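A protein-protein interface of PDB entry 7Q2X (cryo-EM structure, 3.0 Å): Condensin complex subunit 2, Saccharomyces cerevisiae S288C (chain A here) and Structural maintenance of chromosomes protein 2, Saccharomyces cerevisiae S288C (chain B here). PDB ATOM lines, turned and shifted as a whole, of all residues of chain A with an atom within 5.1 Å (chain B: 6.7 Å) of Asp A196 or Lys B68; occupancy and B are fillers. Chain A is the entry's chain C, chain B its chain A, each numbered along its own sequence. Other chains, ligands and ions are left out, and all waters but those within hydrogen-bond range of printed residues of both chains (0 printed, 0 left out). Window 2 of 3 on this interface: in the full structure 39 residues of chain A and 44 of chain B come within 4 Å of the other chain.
The side-chain hydroxyl (OH) of Tyr B67 lies close to the side-chain carboxylate (OD2) of Asp A196 (3.3 Å). The side-chain amino group of Lys B68 lies within salt-bridge range of the side-chain carboxylate of Asp A196. The backbone carbonyl oxygen of Gly A198 lies close to the side-chain carboxylate of Asp B1162, 2.9 Å away.
The backbone carbonyl oxygen of Gly B10 lies within hydrogen-bond range of the backbone NH of Tyr B67 (3.3 Å). The side-chain hydroxyl of Tyr B67 lies within hydrogen-bond range of the side-chain amino group of Lys B68. OH of Tyr B67 sits close to O of Gly B1163 (3.3 Å). The backbone carbonyl oxygen (O) of Arg B69 is in hydrogen-bond range of the side-chain amide nitrogen (NE2) of Gln B71, 2.9 Å away.
Leu A192 touches Gln B71. Leu A192 touches Ala B72. N of Gly B73 touches CD2 of Leu A192, at 3.6 Å. O of Gly B73 touches CG2 of Val A193, 3.8 Å away. OD2 of Asp A196 touches CB of Ala B72 (3.2 Å). Asp B1162 touches Glu A197.
Asp A196 touches three residues of chain B. Printed residues of chain B within 4 Å of Glu A197: Asp B1162 (3.5 Å). Lys B68 touches just one residue of chain A: Asp A196 (2.8 Å). Of the printed residues of chain A, Asp B1162 touches Glu A197 (3.5 Å) and Gly A198 (2.9 Å). The nearest residue of chain B that does not touch Asp A196 is Gly B1163 (5.2 Å). The nearest printed residue of chain A that does not touch Lys B68 is Glu A197 (7.2 Å). The nearest printed residue of chain A that does not touch Ala B72 is Val A193 (4.3 Å).
Hydrophobic or aromatic side chains of chain A within 4 Å of the printed part of chain B: Leu A192 and Val A193. Along chain A the printed residues that touch a printed residue of chain B span positions 192 to 198. Hydrophobic or aromatic side chains of chain B that line the printed part of chain A: Tyr B67 and Ala B72. Along chain B the printed residues that touch a printed residue of chain A span positions 67 to 1162. Among the printed residues, Asp or Glu carboxylates within 4 Å of a Lys or Arg side-chain nitrogen of the other chain: Asp A196 with Lys B68 (2.8 Å).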
ATOM      1  N   ALA A 191     -13.219 -20.489 -15.342  1.00  0.00           N
ATOM      2  CA  ALA A 191     -11.836 -20.402 -14.884  1.00  0.00           C
ATOM      3  C   ALA A 191     -11.757 -20.445 -13.365  1.00  0.00           C
ATOM      4  O   ALA A 191     -10.867 -21.091 -12.801  1.00  0.00           O
ATOM      5  CB  ALA A 191     -11.184 -19.128 -15.423  1.00  0.00           C
ATOM      6  N   LEU A 192     -12.679 -19.761 -12.685  1.00  0.00           N
ATOM      7  CA  LEU A 192     -12.708 -19.788 -11.227  1.00  0.00           C
ATOM      8  C   LEU A 192     -12.991 -21.190 -10.704  1.00  0.00           C
ATOM      9  O   LEU A 192     -12.377 -21.630  -9.726  1.00  0.00           O
ATOM     10  CB  LEU A 192     -13.755 -18.800 -10.711  1.00  0.00           C
ATOM     11  CG  LEU A 192     -13.672 -18.384  -9.243  1.00  0.00           C
ATOM     12  CD1 LEU A 192     -12.277 -17.899  -8.893  1.00  0.00           C
ATOM     13  CD2 LEU A 192     -14.705 -17.309  -8.952  1.00  0.00           C
ATOM     14  N   VAL A 193     -13.922 -21.905 -11.340  1.00  0.00           N
ATOM     15  CA  VAL A 193     -14.233 -23.270 -10.917  1.00  0.00           C
ATOM     16  C   VAL A 193     -13.017 -24.172 -11.103  1.00  0.00           C
ATOM     17  O   VAL A 193     -12.661 -24.961 -10.217  1.00  0.00           O
ATOM     18  CB  VAL A 193     -15.457 -23.802 -11.683  1.00  0.00           C
ATOM     19  CG1 VAL A 193     -15.553 -25.315 -11.555  1.00  0.00           C
ATOM     20  CG2 VAL A 193     -16.728 -23.139 -11.175  1.00  0.00           C
ATOM     21  N   ASP A 194     -12.355 -24.059 -12.258  1.00  0.00           N
ATOM     22  CA  ASP A 194     -11.166 -24.868 -12.509  1.00  0.00           C
ATOM     23  C   ASP A 194     -10.062 -24.550 -11.508  1.00  0.00           C
ATOM     24  O   ASP A 194      -9.383 -25.456 -11.013  1.00  0.00           O
ATOM     25  CB  ASP A 194     -10.675 -24.650 -13.940  1.00  0.00           C
ATOM     26  CG  ASP A 194     -11.591 -25.276 -14.973  1.00  0.00           C
ATOM     27  OD1 ASP A 194     -12.807 -25.377 -14.707  1.00  0.00           O
ATOM     28  OD2 ASP A 194     -11.095 -25.666 -16.050  1.00  0.00           O
ATOM     29  N   PHE A 195      -9.874 -23.266 -11.197  1.00  0.00           N
ATOM     30  CA  PHE A 195      -8.864 -22.868 -10.223  1.00  0.00           C
ATOM     31  C   PHE A 195      -9.190 -23.401  -8.834  1.00  0.00           C
ATOM     32  O   PHE A 195      -8.296 -23.846  -8.105  1.00  0.00           O
ATOM     33  CB  PHE A 195      -8.743 -21.344 -10.210  1.00  0.00           C
ATOM     34  CG  PHE A 195      -7.737 -20.819  -9.232  1.00  0.00           C
ATOM     35  CD1 PHE A 195      -6.389 -20.815  -9.539  1.00  0.00           C
ATOM     36  CD2 PHE A 195      -8.144 -20.309  -8.011  1.00  0.00           C
ATOM     37  CE1 PHE A 195      -5.465 -20.323  -8.641  1.00  0.00           C
ATOM     38  CE2 PHE A 195      -7.224 -19.817  -7.111  1.00  0.00           C
ATOM     39  CZ  PHE A 195      -5.885 -19.823  -7.428  1.00  0.00           C
ATOM     40  N   ASP A 196     -10.467 -23.364  -8.448  1.00  0.00           N
ATOM     41  CA  ASP A 196     -10.876 -23.837  -7.134  1.00  0.00           C
ATOM     42  C   ASP A 196     -10.991 -25.353  -7.061  1.00  0.00           C
ATOM     43  O   ASP A 196     -11.235 -25.887  -5.974  1.00  0.00           O
ATOM     44  CB  ASP A 196     -12.211 -23.207  -6.734  1.00  0.00           C
ATOM     45  CG  ASP A 196     -12.328 -22.998  -5.238  1.00  0.00           C
ATOM     46  OD1 ASP A 196     -11.283 -22.986  -4.554  1.00  0.00           O
ATOM     47  OD2 ASP A 196     -13.466 -22.855  -4.742  1.00  0.00           O
ATOM     48  N   GLU A 197     -10.843 -26.052  -8.190  1.00  0.00           N
ATOM     49  CA  GLU A 197     -10.817 -27.511  -8.154  1.00  0.00           C
ATOM     50  C   GLU A 197      -9.715 -28.014  -7.228  1.00  0.00           C
ATOM     51  O   GLU A 197      -9.931 -28.925  -6.422  1.00  0.00           O
ATOM     52  CB  GLU A 197     -10.632 -28.066  -9.568  1.00  0.00           C
ATOM     53  CG  GLU A 197     -10.634 -29.585  -9.651  1.00  0.00           C
ATOM     54  CD  GLU A 197     -11.969 -30.194  -9.269  1.00  0.00           C
ATOM     55  OE1 GLU A 197     -13.004 -29.507  -9.411  1.00  0.00           O
ATOM     56  OE2 GLU A 197     -11.986 -31.362  -8.827  1.00  0.00           O
ATOM     57  N   GLY A 198      -8.526 -27.421  -7.328  1.00  0.00           N
ATOM     58  CA  GLY A 198      -7.447 -27.692  -6.399  1.00  0.00           C
ATOM     59  C   GLY A 198      -6.960 -29.126  -6.371  1.00  0.00           C
ATOM     60  O   GLY A 198      -7.121 -29.822  -5.364  1.00  0.00           O
ATOM     61  N   GLY B  10     -23.950 -27.760  -3.845  1.00  0.00           N
ATOM     62  CA  GLY B  10     -23.467 -26.423  -3.566  1.00  0.00           C
ATOM     63  C   GLY B  10     -23.704 -25.929  -2.160  1.00  0.00           C
ATOM     64  O   GLY B  10     -23.690 -24.717  -1.932  1.00  0.00           O
ATOM     65  N   LYS B  12     -22.398 -25.656   1.573  1.00  0.00           N
ATOM     66  CA  LYS B  12     -21.266 -25.724   2.503  1.00  0.00           C
ATOM     67  C   LYS B  12     -20.129 -26.482   1.827  1.00  0.00           C
ATOM     68  O   LYS B  12     -19.698 -26.065   0.738  1.00  0.00           O
ATOM     69  CB  LYS B  12     -21.762 -26.307   3.827  1.00  0.00           C
ATOM     70  CG  LYS B  12     -22.748 -25.418   4.562  1.00  0.00           C
ATOM     71  CD  LYS B  12     -23.036 -25.945   5.957  1.00  0.00           C
ATOM     72  CE  LYS B  12     -22.871 -24.861   7.005  1.00  0.00           C
ATOM     73  NZ  LYS B  12     -22.784 -25.433   8.375  1.00  0.00           N
ATOM     74  N   GLN B  63     -26.336 -16.249   2.918  1.00  0.00           N
ATOM     75  CA  GLN B  63     -25.166 -16.111   2.057  1.00  0.00           C
ATOM     76  C   GLN B  63     -24.046 -17.054   2.475  1.00  0.00           C
ATOM     77  O   GLN B  63     -23.333 -17.588   1.619  1.00  0.00           O
ATOM     78  CB  GLN B  63     -24.673 -14.663   2.072  1.00  0.00           C
ATOM     79  CG  GLN B  63     -23.659 -14.335   0.987  1.00  0.00           C
ATOM     80  CD  GLN B  63     -24.311 -13.946  -0.325  1.00  0.00           C
ATOM     81  OE1 GLN B  63     -25.184 -14.650  -0.833  1.00  0.00           O
ATOM     82  NE2 GLN B  63     -23.888 -12.818  -0.882  1.00  0.00           N
ATOM     83  N   ASP B  64     -23.877 -17.274   3.781  1.00  0.00           N
ATOM     84  CA  ASP B  64     -22.852 -18.193   4.259  1.00  0.00           C
ATOM     85  C   ASP B  64     -23.182 -19.645   3.938  1.00  0.00           C
ATOM     86  O   ASP B  64     -22.303 -20.505   4.050  1.00  0.00           O
ATOM     87  CB  ASP B  64     -22.654 -18.022   5.765  1.00  0.00           C
ATOM     88  CG  ASP B  64     -21.868 -16.774   6.111  1.00  0.00           C
ATOM     89  OD1 ASP B  64     -21.929 -15.797   5.334  1.00  0.00           O
ATOM     90  OD2 ASP B  64     -21.189 -16.766   7.160  1.00  0.00           O
ATOM     91  N   LEU B  65     -24.424 -19.939   3.549  1.00  0.00           N
ATOM     92  CA  LEU B  65     -24.809 -21.306   3.230  1.00  0.00           C
ATOM     93  C   LEU B  65     -24.280 -21.765   1.879  1.00  0.00           C
ATOM     94  O   LEU B  65     -24.214 -22.974   1.634  1.00  0.00           O
ATOM     95  CB  LEU B  65     -26.332 -21.440   3.257  1.00  0.00           C
ATOM     96  CG  LEU B  65     -26.928 -22.042   4.530  1.00  0.00           C
ATOM     97  CD1 LEU B  65     -26.478 -21.266   5.751  1.00  0.00           C
ATOM     98  CD2 LEU B  65     -28.437 -22.062   4.445  1.00  0.00           C
ATOM     99  N   ILE B  66     -23.902 -20.832   1.002  1.00  0.00           N
ATOM    100  CA  ILE B  66     -23.314 -21.206  -0.277  1.00  0.00           C
ATOM    101  C   ILE B  66     -21.943 -21.839  -0.044  1.00  0.00           C
ATOM    102  O   ILE B  66     -21.367 -21.763   1.048  1.00  0.00           O
ATOM    103  CB  ILE B  66     -23.226 -19.980  -1.203  1.00  0.00           C
ATOM    104  CG1 ILE B  66     -24.521 -19.171  -1.126  1.00  0.00           C
ATOM    105  CG2 ILE B  66     -23.017 -20.391  -2.654  1.00  0.00           C
ATOM    106  CD1 ILE B  66     -24.438 -17.816  -1.797  1.00  0.00           C
ATOM    107  N   TYR B  67     -21.424 -22.494  -1.087  1.00  0.00           N
ATOM    108  CA  TYR B  67     -20.148 -23.195  -0.976  1.00  0.00           C
ATOM    109  C   TYR B  67     -19.037 -22.267  -0.503  1.00  0.00           C
ATOM    110  O   TYR B  67     -18.248 -22.622   0.378  1.00  0.00           O
ATOM    111  CB  TYR B  67     -19.783 -23.831  -2.317  1.00  0.00           C
ATOM    112  CG  TYR B  67     -18.328 -24.230  -2.429  1.00  0.00           C
ATOM    113  CD1 TYR B  67     -17.767 -25.147  -1.548  1.00  0.00           C
ATOM    114  CD2 TYR B  67     -17.517 -23.693  -3.418  1.00  0.00           C
ATOM    115  CE1 TYR B  67     -16.440 -25.512  -1.648  1.00  0.00           C
ATOM    116  CE2 TYR B  67     -16.189 -24.053  -3.526  1.00  0.00           C
ATOM    117  CZ  TYR B  67     -15.655 -24.962  -2.639  1.00  0.00           C
ATOM    118  OH  TYR B  67     -14.331 -25.323  -2.743  1.00  0.00           O
ATOM    119  N   LYS B  68     -18.944 -21.077  -1.089  1.00  0.00           N
ATOM    120  CA  LYS B  68     -17.984 -20.076  -0.636  1.00  0.00           C
ATOM    121  C   LYS B  68     -18.614 -18.691  -0.654  1.00  0.00           C
ATOM    122  O   LYS B  68     -18.009 -17.720  -1.121  1.00  0.00           O
ATOM    123  CB  LYS B  68     -16.707 -20.113  -1.473  1.00  0.00           C
ATOM    124  CG  LYS B  68     -15.680 -21.113  -0.959  1.00  0.00           C
ATOM    125  CD  LYS B  68     -14.381 -21.045  -1.739  1.00  0.00           C
ATOM    126  CE  LYS B  68     -13.286 -21.847  -1.055  1.00  0.00           C
ATOM    127  NZ  LYS B  68     -12.464 -22.610  -2.033  1.00  0.00           N
ATOM    128  N   ARG B  69     -19.845 -18.591  -0.148  1.00  0.00           N
ATOM    129  CA  ARG B  69     -20.598 -17.335  -0.108  1.00  0.00           C
ATOM    130  C   ARG B  69     -20.777 -16.746  -1.505  1.00  0.00           C
ATOM    131  O   ARG B  69     -20.764 -15.528  -1.694  1.00  0.00           O
ATOM    132  CB  ARG B  69     -19.937 -16.321   0.831  1.00  0.00           C
ATOM    133  CG  ARG B  69     -19.521 -16.896   2.176  1.00  0.00           C
ATOM    134  CD  ARG B  69     -18.887 -15.857   3.103  1.00  0.00           C
ATOM    135  NE  ARG B  69     -19.842 -14.879   3.612  1.00  0.00           N
ATOM    136  CZ  ARG B  69     -20.143 -13.731   3.019  1.00  0.00           C
ATOM    137  NH1 ARG B  69     -19.537 -13.346   1.907  1.00  0.00           N
ATOM    138  NH2 ARG B  69     -21.065 -12.942   3.563  1.00  0.00           N
ATOM    139  N   GLY B  70     -20.956 -17.620  -2.492  1.00  0.00           N
ATOM    140  CA  GLY B  70     -21.156 -17.173  -3.862  1.00  0.00           C
ATOM    141  C   GLY B  70     -19.982 -16.417  -4.442  1.00  0.00           C
ATOM    142  O   GLY B  70     -20.175 -15.407  -5.130  1.00  0.00           O
ATOM    143  N   GLN B  71     -18.759 -16.881  -4.177  1.00  0.00           N
ATOM    144  CA  GLN B  71     -17.562 -16.206  -4.651  1.00  0.00           C
ATOM    145  C   GLN B  71     -16.592 -17.108  -5.400  1.00  0.00           C
ATOM    146  O   GLN B  71     -15.569 -16.610  -5.882  1.00  0.00           O
ATOM    147  CB  GLN B  71     -16.813 -15.550  -3.477  1.00  0.00           C
ATOM    148  CG  GLN B  71     -17.676 -14.734  -2.510  1.00  0.00           C
ATOM    149  CD  GLN B  71     -18.475 -13.617  -3.174  1.00  0.00           C
ATOM    150  OE1 GLN B  71     -18.273 -13.289  -4.344  1.00  0.00           O
ATOM    151  NE2 GLN B  71     -19.391 -13.026  -2.417  1.00  0.00           N
ATOM    152  N   ALA B  72     -16.872 -18.403  -5.519  1.00  0.00           N
ATOM    153  CA  ALA B  72     -15.950 -19.349  -6.142  1.00  0.00           C
ATOM    154  C   ALA B  72     -16.660 -20.172  -7.208  1.00  0.00           C
ATOM    155  O   ALA B  72     -16.515 -21.392  -7.291  1.00  0.00           O
ATOM    156  CB  ALA B  72     -15.315 -20.257  -5.096  1.00  0.00           C
ATOM    157  N   GLY B  73     -17.446 -19.502  -8.047  1.00  0.00           N
ATOM    158  CA  GLY B  73     -18.116 -20.171  -9.141  1.00  0.00           C
ATOM    159  C   GLY B  73     -19.325 -20.990  -8.754  1.00  0.00           C
ATOM    160  O   GLY B  73     -19.856 -21.716  -9.602  1.00  0.00           O
ATOM    161  N   VAL B  74     -19.773 -20.907  -7.506  1.00  0.00           N
ATOM    162  CA  VAL B  74     -20.964 -21.606  -7.038  1.00  0.00           C
ATOM    163  C   VAL B  74     -21.971 -20.556  -6.594  1.00  0.00           C
ATOM    164  O   VAL B  74     -21.671 -19.725  -5.728  1.00  0.00           O
ATOM    165  CB  VAL B  74     -20.642 -22.584  -5.899  1.00  0.00           C
ATOM    166  CG1 VAL B  74     -21.920 -23.198  -5.350  1.00  0.00           C
ATOM    167  CG2 VAL B  74     -19.689 -23.665  -6.382  1.00  0.00           C
ATOM    168  N   ASP B1162     -11.172 -33.058  -2.773  1.00  0.00           N
ATOM    169  CA  ASP B1162     -10.687 -31.832  -3.420  1.00  0.00           C
ATOM    170  C   ASP B1162     -11.751 -30.751  -3.240  1.00  0.00           C
ATOM    171  O   ASP B1162     -12.659 -30.618  -4.064  1.00  0.00           O
ATOM    172  CB  ASP B1162     -10.374 -32.074  -4.890  1.00  0.00           C
ATOM    173  CG  ASP B1162      -9.015 -32.712  -5.099  1.00  0.00           C
ATOM    174  OD1 ASP B1162      -8.066 -32.343  -4.375  1.00  0.00           O
ATOM    175  OD2 ASP B1162      -8.895 -33.580  -5.989  1.00  0.00           O
ATOM    176  N   GLY B1163     -11.625 -29.976  -2.164  1.00  0.00           N
ATOM    177  CA  GLY B1163     -12.552 -28.889  -1.900  1.00  0.00           C
ATOM    178  C   GLY B1163     -14.001 -29.297  -1.766  1.00  0.00           C
ATOM    179  O   GLY B1163     -14.871 -28.429  -1.654  1.00  0.00           O
